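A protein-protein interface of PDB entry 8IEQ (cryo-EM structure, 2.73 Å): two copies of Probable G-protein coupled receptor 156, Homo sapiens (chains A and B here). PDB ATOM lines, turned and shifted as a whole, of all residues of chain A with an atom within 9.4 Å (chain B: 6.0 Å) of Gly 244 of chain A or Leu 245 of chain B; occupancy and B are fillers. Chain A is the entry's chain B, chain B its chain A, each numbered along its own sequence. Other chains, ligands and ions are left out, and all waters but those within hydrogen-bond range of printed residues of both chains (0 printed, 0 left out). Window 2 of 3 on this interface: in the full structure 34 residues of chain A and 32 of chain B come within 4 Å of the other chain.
Tyr 241 of chain A touches Ala 243 of chain B, and with the chains exchanged Ala 243 of chain A touches Tyr 241 of chain B.
Tyr 241 of chain A touches Gly 244 of chain B, and with the chains exchanged Gly 244 of chain A touches Tyr 241 of chain B.
Gly 244 of chain A touches its own counterpart, Gly 244 of chain B.
Gly 244 of chain A touches Leu 245 of chain B, and with the chains exchanged Leu 245 of chain A touches Gly 244 of chain B.
Positions printed for both chains: 146, 240, 241, 242, 243, 244, 245, 246, 247 and 249.
Of the 12 pairs that touch across the chains among the printed residues, 9 have their exchanged pair printed and touching as well.
Printed residues of chain B within 4 Å of Ala 240 of chain A: Tyr 241.
Gly 244 of chain A touches just these residues of chain B: Tyr 241, Gly 244 and Leu 245.
Ser 257 of chain A touches none of the printed residues of chain B.
Printed residues of chain B within 4 Å of Met 261 of chain A: Tyr 241 (3.5 Å).
Gly 244 of chain B touches just these residues of chain A: Tyr 241, Gly 244 and Leu 245.
No residue of chain A comes within 4 Å of Thr 246 of chain B.
Val 249 of chain B touches none of the printed residues of chain A.
The nearest residue of chain B that does not touch Gly 244 of chain A is Ala 240 of chain B (5.3 Å).
The nearest residue of chain A that does not touch Leu 245 of chain B is Leu 245 of chain A (4.1 Å).
Of the 22 printed residues of chain A, 8 touch a printed residue of chain B.
Printed residues of chain A that touch a printed residue of chain B: Leu 237, Ala 240, Tyr 241, Ala 243, Gly 244, Leu 245, His 248 and Met 261.
Hydrophobic or aromatic side chains of chain A that line the printed part of chain B: Tyr 241, Leu 245, His 248 and Met 261.
Among the printed residues, 12 pairs touch across the chains.
Among the printed residues, no Asp or Glu carboxylate lies within 4 Å of a Lys or Arg side-chain nitrogen of the other chain.
NE2 of His 248 of chain A lies within hydrogen-bond range of OH of Tyr 146 of chain B, 3.1 Å away.
The backbone carbonyl oxygen (O) of Gly 244 of chain B sits close to the backbone NH (N) of Leu 245 of chain A, at 3.5 Å.
N of Leu 245 of chain B sits close to O of Gly 244 of chain A, 3.5 Å away.
The backbone carbonyl oxygen (O) of Gly 244 of chain A sits close to the backbone carbonyl oxygen (O) of Gly 244 of chain B, 3.5 Å away.
CB of Ala 240 of chain B touches O of Leu 237 of chain A, 3.7 Å away.
O of Ala 240 of chain A touches CA of Tyr 241 of chain B, 3.6 Å away.
Ala 240 of chain B touches Tyr 241 of chain A.
Tyr 241 of chain A touches Ala 243 of chain B.
Tyr 241 of chain A touches Gly 244 of chain B.
Tyr 241 of chain B touches Ala 243 of chain A (CE1 to O, 3.9 Å).
Gly 244 of chain A touches Tyr 241 of chain B (N to CD1, 3.5 Å).
Met 261 of chain A touches Tyr 241 of chain B.
O of Ala 243 of chain A lies within hydrogen-bond range of OG of Ser 257 of chain A (2.6 Å).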
ATOM      1  N   SER A 142     -10.387   3.714 -23.099  1.00  0.00           N
ATOM      2  CA  SER A 142      -9.365   4.493 -22.408  1.00  0.00           C
ATOM      3  C   SER A 142      -8.384   3.590 -21.670  1.00  0.00           C
ATOM      4  O   SER A 142      -7.174   3.839 -21.685  1.00  0.00           O
ATOM      5  CB  SER A 142     -10.014   5.477 -21.439  1.00  0.00           C
ATOM      6  OG  SER A 142     -10.673   6.510 -22.144  1.00  0.00           O
ATOM      7  N   TYR A 146      -4.406   3.236 -22.313  1.00  0.00           N
ATOM      8  CA  TYR A 146      -3.458   3.459 -21.228  1.00  0.00           C
ATOM      9  C   TYR A 146      -2.514   2.274 -21.067  1.00  0.00           C
ATOM     10  O   TYR A 146      -1.310   2.457 -20.850  1.00  0.00           O
ATOM     11  CB  TYR A 146      -4.216   3.721 -19.929  1.00  0.00           C
ATOM     12  CG  TYR A 146      -3.367   3.619 -18.685  1.00  0.00           C
ATOM     13  CD1 TYR A 146      -2.403   4.574 -18.400  1.00  0.00           C
ATOM     14  CD2 TYR A 146      -3.530   2.568 -17.796  1.00  0.00           C
ATOM     15  CE1 TYR A 146      -1.627   4.485 -17.265  1.00  0.00           C
ATOM     16  CE2 TYR A 146      -2.756   2.470 -16.660  1.00  0.00           C
ATOM     17  CZ  TYR A 146      -1.806   3.432 -16.400  1.00  0.00           C
ATOM     18  OH  TYR A 146      -1.033   3.339 -15.267  1.00  0.00           O
ATOM     19  N   LEU A 236     -17.635   6.239 -12.494  1.00  0.00           N
ATOM     20  CA  LEU A 236     -17.346   7.451 -13.252  1.00  0.00           C
ATOM     21  C   LEU A 236     -16.154   8.209 -12.682  1.00  0.00           C
ATOM     22  O   LEU A 236     -15.454   8.896 -13.428  1.00  0.00           O
ATOM     23  CB  LEU A 236     -18.579   8.355 -13.285  1.00  0.00           C
ATOM     24  CG  LEU A 236     -19.425   8.271 -14.560  1.00  0.00           C
ATOM     25  CD1 LEU A 236     -20.031   6.890 -14.756  1.00  0.00           C
ATOM     26  CD2 LEU A 236     -20.517   9.319 -14.526  1.00  0.00           C
ATOM     27  N   LEU A 237     -15.904   8.101 -11.377  1.00  0.00           N
ATOM     28  CA  LEU A 237     -14.670   8.640 -10.820  1.00  0.00           C
ATOM     29  C   LEU A 237     -13.463   7.895 -11.368  1.00  0.00           C
ATOM     30  O   LEU A 237     -12.450   8.512 -11.724  1.00  0.00           O
ATOM     31  CB  LEU A 237     -14.697   8.556  -9.295  1.00  0.00           C
ATOM     32  CG  LEU A 237     -15.454   9.656  -8.552  1.00  0.00           C
ATOM     33  CD1 LEU A 237     -15.697   9.228  -7.119  1.00  0.00           C
ATOM     34  CD2 LEU A 237     -14.698  10.971  -8.592  1.00  0.00           C
ATOM     35  N   TYR A 238     -13.552   6.567 -11.454  1.00  0.00           N
ATOM     36  CA  TYR A 238     -12.471   5.830 -12.102  1.00  0.00           C
ATOM     37  C   TYR A 238     -12.360   6.188 -13.580  1.00  0.00           C
ATOM     38  O   TYR A 238     -11.256   6.203 -14.131  1.00  0.00           O
ATOM     39  CB  TYR A 238     -12.664   4.323 -11.943  1.00  0.00           C
ATOM     40  CG  TYR A 238     -11.484   3.527 -12.456  1.00  0.00           C
ATOM     41  CD1 TYR A 238     -10.218   3.694 -11.912  1.00  0.00           C
ATOM     42  CD2 TYR A 238     -11.633   2.620 -13.495  1.00  0.00           C
ATOM     43  CE1 TYR A 238      -9.140   2.979 -12.382  1.00  0.00           C
ATOM     44  CE2 TYR A 238     -10.558   1.899 -13.969  1.00  0.00           C
ATOM     45  CZ  TYR A 238      -9.314   2.083 -13.409  1.00  0.00           C
ATOM     46  OH  TYR A 238      -8.238   1.368 -13.877  1.00  0.00           O
ATOM     47  N   GLY A 239     -13.483   6.478 -14.234  1.00  0.00           N
ATOM     48  CA  GLY A 239     -13.430   6.919 -15.618  1.00  0.00           C
ATOM     49  C   GLY A 239     -12.740   8.259 -15.780  1.00  0.00           C
ATOM     50  O   GLY A 239     -11.994   8.469 -16.737  1.00  0.00           O
ATOM     51  N   ALA A 240     -12.988   9.188 -14.858  1.00  0.00           N
ATOM     52  CA  ALA A 240     -12.281  10.466 -14.877  1.00  0.00           C
ATOM     53  C   ALA A 240     -10.793  10.270 -14.621  1.00  0.00           C
ATOM     54  O   ALA A 240      -9.955  10.946 -15.229  1.00  0.00           O
ATOM     55  CB  ALA A 240     -12.883  11.414 -13.842  1.00  0.00           C
ATOM     56  N   TYR A 241     -10.448   9.347 -13.722  1.00  0.00           N
ATOM     57  CA  TYR A 241      -9.044   9.014 -13.504  1.00  0.00           C
ATOM     58  C   TYR A 241      -8.401   8.473 -14.778  1.00  0.00           C
ATOM     59  O   TYR A 241      -7.278   8.851 -15.123  1.00  0.00           O
ATOM     60  CB  TYR A 241      -8.927   7.999 -12.368  1.00  0.00           C
ATOM     61  CG  TYR A 241      -7.510   7.650 -11.978  1.00  0.00           C
ATOM     62  CD1 TYR A 241      -6.648   8.616 -11.485  1.00  0.00           C
ATOM     63  CD2 TYR A 241      -7.038   6.353 -12.097  1.00  0.00           C
ATOM     64  CE1 TYR A 241      -5.359   8.302 -11.124  1.00  0.00           C
ATOM     65  CE2 TYR A 241      -5.749   6.030 -11.741  1.00  0.00           C
ATOM     66  CZ  TYR A 241      -4.913   7.008 -11.255  1.00  0.00           C
ATOM     67  OH  TYR A 241      -3.624   6.693 -10.896  1.00  0.00           O
ATOM     68  N   LEU A 242      -9.102   7.584 -15.485  1.00  0.00           N
ATOM     69  CA  LEU A 242      -8.580   7.043 -16.737  1.00  0.00           C
ATOM     70  C   LEU A 242      -8.453   8.123 -17.804  1.00  0.00           C
ATOM     71  O   LEU A 242      -7.494   8.125 -18.582  1.00  0.00           O
ATOM     72  CB  LEU A 242      -9.483   5.917 -17.240  1.00  0.00           C
ATOM     73  CG  LEU A 242      -9.211   4.502 -16.735  1.00  0.00           C
ATOM     74  CD1 LEU A 242     -10.293   3.567 -17.238  1.00  0.00           C
ATOM     75  CD2 LEU A 242      -7.840   4.012 -17.172  1.00  0.00           C
ATOM     76  N   ALA A 243      -9.425   9.032 -17.874  1.00  0.00           N
ATOM     77  CA  ALA A 243      -9.347  10.131 -18.828  1.00  0.00           C
ATOM     78  C   ALA A 243      -8.148  11.020 -18.540  1.00  0.00           C
ATOM     79  O   ALA A 243      -7.470  11.477 -19.466  1.00  0.00           O
ATOM     80  CB  ALA A 243     -10.639  10.945 -18.795  1.00  0.00           C
ATOM     81  N   GLY A 244      -7.879  11.290 -17.263  1.00  0.00           N
ATOM     82  CA  GLY A 244      -6.697  12.060 -16.915  1.00  0.00           C
ATOM     83  C   GLY A 244      -5.409  11.323 -17.225  1.00  0.00           C
ATOM     84  O   GLY A 244      -4.443  11.920 -17.707  1.00  0.00           O
ATOM     85  N   LEU A 245      -5.372  10.018 -16.949  1.00  0.00           N
ATOM     86  CA  LEU A 245      -4.175   9.227 -17.209  1.00  0.00           C
ATOM     87  C   LEU A 245      -3.814   9.194 -18.684  1.00  0.00           C
ATOM     88  O   LEU A 245      -2.633   9.045 -19.016  1.00  0.00           O
ATOM     89  CB  LEU A 245      -4.368   7.791 -16.713  1.00  0.00           C
ATOM     90  CG  LEU A 245      -3.917   7.460 -15.291  1.00  0.00           C
ATOM     91  CD1 LEU A 245      -4.404   6.076 -14.922  1.00  0.00           C
ATOM     92  CD2 LEU A 245      -2.408   7.557 -15.139  1.00  0.00           C
ATOM     93  N   THR A 246      -4.799   9.327 -19.568  1.00  0.00           N
ATOM     94  CA  THR A 246      -4.586   9.251 -21.004  1.00  0.00           C
ATOM     95  C   THR A 246      -4.872  10.618 -21.614  1.00  0.00           C
ATOM     96  O   THR A 246      -5.416  10.716 -22.717  1.00  0.00           O
ATOM     97  CB  THR A 246      -5.486   8.171 -21.611  1.00  0.00           C
ATOM     98  OG1 THR A 246      -5.472   7.011 -20.773  1.00  0.00           O
ATOM     99  CG2 THR A 246      -4.993   7.756 -22.976  1.00  0.00           C
ATOM    100  N   GLY A 247      -4.502  11.675 -20.896  1.00  0.00           N
ATOM    101  CA  GLY A 247      -4.894  13.027 -21.244  1.00  0.00           C
ATOM    102  C   GLY A 247      -4.401  13.512 -22.590  1.00  0.00           C
ATOM    103  O   GLY A 247      -5.171  14.088 -23.364  1.00  0.00           O
ATOM    104  N   HIS A 248      -3.122  13.293 -22.878  1.00  0.00           N
ATOM    105  CA  HIS A 248      -2.481  13.748 -24.109  1.00  0.00           C
ATOM    106  C   HIS A 248      -1.657  12.625 -24.718  1.00  0.00           C
ATOM    107  O   HIS A 248      -0.494  12.800 -25.086  1.00  0.00           O
ATOM    108  CB  HIS A 248      -1.613  14.974 -23.842  1.00  0.00           C
ATOM    109  CG  HIS A 248      -2.322  16.068 -23.103  1.00  0.00           C
ATOM    110  ND1 HIS A 248      -3.255  16.887 -23.701  1.00  0.00           N
ATOM    111  CD2 HIS A 248      -2.236  16.473 -21.813  1.00  0.00           C
ATOM    112  CE1 HIS A 248      -3.711  17.752 -22.813  1.00  0.00           C
ATOM    113  NE2 HIS A 248      -3.110  17.522 -21.659  1.00  0.00           N
ATOM    114  N   VAL A 249      -2.263  11.444 -24.831  1.00  0.00           N
ATOM    115  CA  VAL A 249      -1.563  10.246 -25.281  1.00  0.00           C
ATOM    116  C   VAL A 249      -1.821   9.994 -26.763  1.00  0.00           C
ATOM    117  O   VAL A 249      -1.042   9.301 -27.426  1.00  0.00           O
ATOM    118  CB  VAL A 249      -1.975   9.028 -24.432  1.00  0.00           C
ATOM    119  CG1 VAL A 249      -1.422   7.737 -25.014  1.00  0.00           C
ATOM    120  CG2 VAL A 249      -1.495   9.203 -23.002  1.00  0.00           C
ATOM    121  N   ASN A 255      -7.918   8.962 -28.519  1.00  0.00           N
ATOM    122  CA  ASN A 255      -8.015   9.437 -27.147  1.00  0.00           C
ATOM    123  C   ASN A 255      -9.450   9.859 -26.843  1.00  0.00           C
ATOM    124  O   ASN A 255     -10.084  10.561 -27.633  1.00  0.00           O
ATOM    125  CB  ASN A 255      -7.052  10.608 -26.942  1.00  0.00           C
ATOM    126  CG  ASN A 255      -7.054  11.137 -25.530  1.00  0.00           C
ATOM    127  OD1 ASN A 255      -7.145  12.342 -25.313  1.00  0.00           O
ATOM    128  ND2 ASN A 255      -6.912  10.246 -24.561  1.00  0.00           N
ATOM    129  N   GLN A 256      -9.962   9.431 -25.684  1.00  0.00           N
ATOM    130  CA  GLN A 256     -11.357   9.639 -25.303  1.00  0.00           C
ATOM    131  C   GLN A 256     -11.483  10.401 -23.987  1.00  0.00           C
ATOM    132  O   GLN A 256     -12.442  10.203 -23.243  1.00  0.00           O
ATOM    133  CB  GLN A 256     -12.091   8.301 -25.204  1.00  0.00           C
ATOM    134  CG  GLN A 256     -12.183   7.521 -26.505  1.00  0.00           C
ATOM    135  CD  GLN A 256     -13.382   7.923 -27.340  1.00  0.00           C
ATOM    136  OE1 GLN A 256     -13.398   8.989 -27.954  1.00  0.00           O
ATOM    137  NE2 GLN A 256     -14.400   7.074 -27.358  1.00  0.00           N
ATOM    138  N   SER A 257     -10.527  11.279 -23.685  1.00  0.00           N
ATOM    139  CA  SER A 257     -10.562  11.991 -22.410  1.00  0.00           C
ATOM    140  C   SER A 257     -11.619  13.090 -22.407  1.00  0.00           C
ATOM    141  O   SER A 257     -12.347  13.253 -21.420  1.00  0.00           O
ATOM    142  CB  SER A 257      -9.183  12.571 -22.105  1.00  0.00           C
ATOM    143  OG  SER A 257      -8.238  11.535 -21.929  1.00  0.00           O
ATOM    144  N   LEU A 258     -11.714  13.859 -23.494  1.00  0.00           N
ATOM    145  CA  LEU A 258     -12.687  14.945 -23.549  1.00  0.00           C
ATOM    146  C   LEU A 258     -14.113  14.418 -23.516  1.00  0.00           C
ATOM    147  O   LEU A 258     -14.971  14.975 -22.820  1.00  0.00           O
ATOM    148  CB  LEU A 258     -12.464  15.786 -24.805  1.00  0.00           C
ATOM    149  CG  LEU A 258     -13.081  17.188 -24.832  1.00  0.00           C
ATOM    150  CD1 LEU A 258     -12.546  18.073 -23.717  1.00  0.00           C
ATOM    151  CD2 LEU A 258     -12.846  17.829 -26.185  1.00  0.00           C
ATOM    152  N   ILE A 260     -15.109  11.633 -22.170  1.00  0.00           N
ATOM    153  CA  ILE A 260     -15.369  11.132 -20.824  1.00  0.00           C
ATOM    154  C   ILE A 260     -15.680  12.285 -19.878  1.00  0.00           C
ATOM    155  O   ILE A 260     -16.624  12.216 -19.085  1.00  0.00           O
ATOM    156  CB  ILE A 260     -14.178  10.297 -20.316  1.00  0.00           C
ATOM    157  CG1 ILE A 260     -14.196   8.912 -20.964  1.00  0.00           C
ATOM    158  CG2 ILE A 260     -14.214  10.163 -18.784  1.00  0.00           C
ATOM    159  CD1 ILE A 260     -12.908   8.133 -20.807  1.00  0.00           C
ATOM    160  N   MET A 261     -14.885  13.354 -19.933  1.00  0.00           N
ATOM    161  CA  MET A 261     -15.081  14.447 -18.986  1.00  0.00           C
ATOM    162  C   MET A 261     -16.402  15.163 -19.236  1.00  0.00           C
ATOM    163  O   MET A 261     -17.162  15.432 -18.292  1.00  0.00           O
ATOM    164  CB  MET A 261     -13.912  15.429 -19.069  1.00  0.00           C
ATOM    165  CG  MET A 261     -12.629  15.003 -18.344  1.00  0.00           C
ATOM    166  SD  MET A 261     -12.816  14.350 -16.668  1.00  0.00           S
ATOM    167  CE  MET A 261     -12.920  15.866 -15.723  1.00  0.00           C
ATOM    168  N   TYR B 146       1.054  19.454 -12.320  1.00  0.00           N
ATOM    169  CA  TYR B 146       0.736  19.299 -13.736  1.00  0.00           C
ATOM    170  C   TYR B 146       1.253  20.474 -14.556  1.00  0.00           C
ATOM    171  O   TYR B 146       1.839  20.280 -15.626  1.00  0.00           O
ATOM    172  CB  TYR B 146      -0.774  19.156 -13.914  1.00  0.00           C
ATOM    173  CG  TYR B 146      -1.228  19.240 -15.349  1.00  0.00           C
ATOM    174  CD1 TYR B 146      -0.910  18.241 -16.256  1.00  0.00           C
ATOM    175  CD2 TYR B 146      -1.968  20.322 -15.799  1.00  0.00           C
ATOM    176  CE1 TYR B 146      -1.320  18.315 -17.568  1.00  0.00           C
ATOM    177  CE2 TYR B 146      -2.382  20.405 -17.108  1.00  0.00           C
ATOM    178  CZ  TYR B 146      -2.055  19.400 -17.989  1.00  0.00           C
ATOM    179  OH  TYR B 146      -2.468  19.482 -19.298  1.00  0.00           O
ATOM    180  N   ALA B 240     -10.211  13.841  -9.612  1.00  0.00           N
ATOM    181  CA  ALA B 240      -9.801  12.557 -10.173  1.00  0.00           C
ATOM    182  C   ALA B 240      -9.127  12.743 -11.524  1.00  0.00           C
ATOM    183  O   ALA B 240      -8.140  12.065 -11.834  1.00  0.00           O
ATOM    184  CB  ALA B 240     -11.010  11.633 -10.300  1.00  0.00           C
ATOM    185  N   TYR B 241      -9.647  13.660 -12.342  1.00  0.00           N
ATOM    186  CA  TYR B 241      -8.987  13.989 -13.601  1.00  0.00           C
ATOM    187  C   TYR B 241      -7.571  14.503 -13.363  1.00  0.00           C
ATOM    188  O   TYR B 241      -6.628  14.084 -14.044  1.00  0.00           O
ATOM    189  CB  TYR B 241      -9.820  15.028 -14.352  1.00  0.00           C
ATOM    190  CG  TYR B 241      -9.288  15.403 -15.715  1.00  0.00           C
ATOM    191  CD1 TYR B 241      -9.217  14.469 -16.738  1.00  0.00           C
ATOM    192  CD2 TYR B 241      -8.872  16.697 -15.981  1.00  0.00           C
ATOM    193  CE1 TYR B 241      -8.738  14.813 -17.983  1.00  0.00           C
ATOM    194  CE2 TYR B 241      -8.393  17.048 -17.222  1.00  0.00           C
ATOM    195  CZ  TYR B 241      -8.328  16.102 -18.219  1.00  0.00           C
ATOM    196  OH  TYR B 241      -7.850  16.451 -19.458  1.00  0.00           O
ATOM    197  N   LEU B 242      -7.404  15.403 -12.394  1.00  0.00           N
ATOM    198  CA  LEU B 242      -6.083  15.949 -12.096  1.00  0.00           C
ATOM    199  C   LEU B 242      -5.149  14.880 -11.542  1.00  0.00           C
ATOM    200  O   LEU B 242      -3.956  14.864 -11.863  1.00  0.00           O
ATOM    201  CB  LEU B 242      -6.203  17.106 -11.106  1.00  0.00           C
ATOM    202  CG  LEU B 242      -6.335  18.512 -11.690  1.00  0.00           C
ATOM    203  CD1 LEU B 242      -6.673  19.490 -10.584  1.00  0.00           C
ATOM    204  CD2 LEU B 242      -5.062  18.933 -12.407  1.00  0.00           C
ATOM    205  N   ALA B 243      -5.667  13.993 -10.692  1.00  0.00           N
ATOM    206  CA  ALA B 243      -4.857  12.902 -10.167  1.00  0.00           C
ATOM    207  C   ALA B 243      -4.388  11.984 -11.286  1.00  0.00           C
ATOM    208  O   ALA B 243      -3.242  11.525 -11.281  1.00  0.00           O
ATOM    209  CB  ALA B 243      -5.649  12.111  -9.128  1.00  0.00           C
ATOM    210  N   GLY B 244      -5.265  11.697 -12.248  1.00  0.00           N
ATOM    211  CA  GLY B 244      -4.847  10.926 -13.405  1.00  0.00           C
ATOM    212  C   GLY B 244      -3.811  11.652 -14.241  1.00  0.00           C
ATOM    213  O   GLY B 244      -2.868  11.038 -14.745  1.00  0.00           O
ATOM    214  N   LEU B 245      -3.971  12.968 -14.402  1.00  0.00           N
ATOM    215  CA  LEU B 245      -3.020  13.732 -15.201  1.00  0.00           C
ATOM    216  C   LEU B 245      -1.625  13.681 -14.594  1.00  0.00           C
ATOM    217  O   LEU B 245      -0.633  13.507 -15.311  1.00  0.00           O
ATOM    218  CB  LEU B 245      -3.484  15.182 -15.333  1.00  0.00           C
ATOM    219  CG  LEU B 245      -4.456  15.521 -16.465  1.00  0.00           C
ATOM    220  CD1 LEU B 245      -4.939  16.949 -16.307  1.00  0.00           C
ATOM    221  CD2 LEU B 245      -3.826  15.321 -17.834  1.00  0.00           C
ATOM    222  N   THR B 246      -1.528  13.835 -13.277  1.00  0.00           N
ATOM    223  CA  THR B 246      -0.256  13.720 -12.567  1.00  0.00           C
ATOM    224  C   THR B 246      -0.038  12.297 -12.066  1.00  0.00           C
ATOM    225  O   THR B 246       0.263  12.070 -10.900  1.00  0.00           O
ATOM    226  CB  THR B 246      -0.216  14.710 -11.409  1.00  0.00           C
ATOM    227  OG1 THR B 246      -1.395  14.560 -10.609  1.00  0.00           O
ATOM    228  CG2 THR B 246      -0.155  16.128 -11.928  1.00  0.00           C
ATOM    229  N   GLY B 247      -0.182  11.322 -12.958  1.00  0.00           N
ATOM    230  CA  GLY B 247      -0.024   9.920 -12.620  1.00  0.00           C
ATOM    231  C   GLY B 247       1.401   9.470 -12.897  1.00  0.00           C
ATOM    232  O   GLY B 247       1.872   9.537 -14.034  1.00  0.00           O
ATOM    233  N   VAL B 249       4.106  10.908 -11.968  1.00  0.00           N
ATOM    234  CA  VAL B 249       4.875  12.081 -12.361  1.00  0.00           C
ATOM    235  C   VAL B 249       5.996  12.376 -11.371  1.00  0.00           C
ATOM    236  O   VAL B 249       7.007  12.970 -11.741  1.00  0.00           O
ATOM    237  CB  VAL B 249       3.940  13.299 -12.532  1.00  0.00           C
ATOM    238  CG1 VAL B 249       4.724  14.614 -12.549  1.00  0.00           C
ATOM    239  CG2 VAL B 249       3.133  13.157 -13.811  1.00  0.00           C
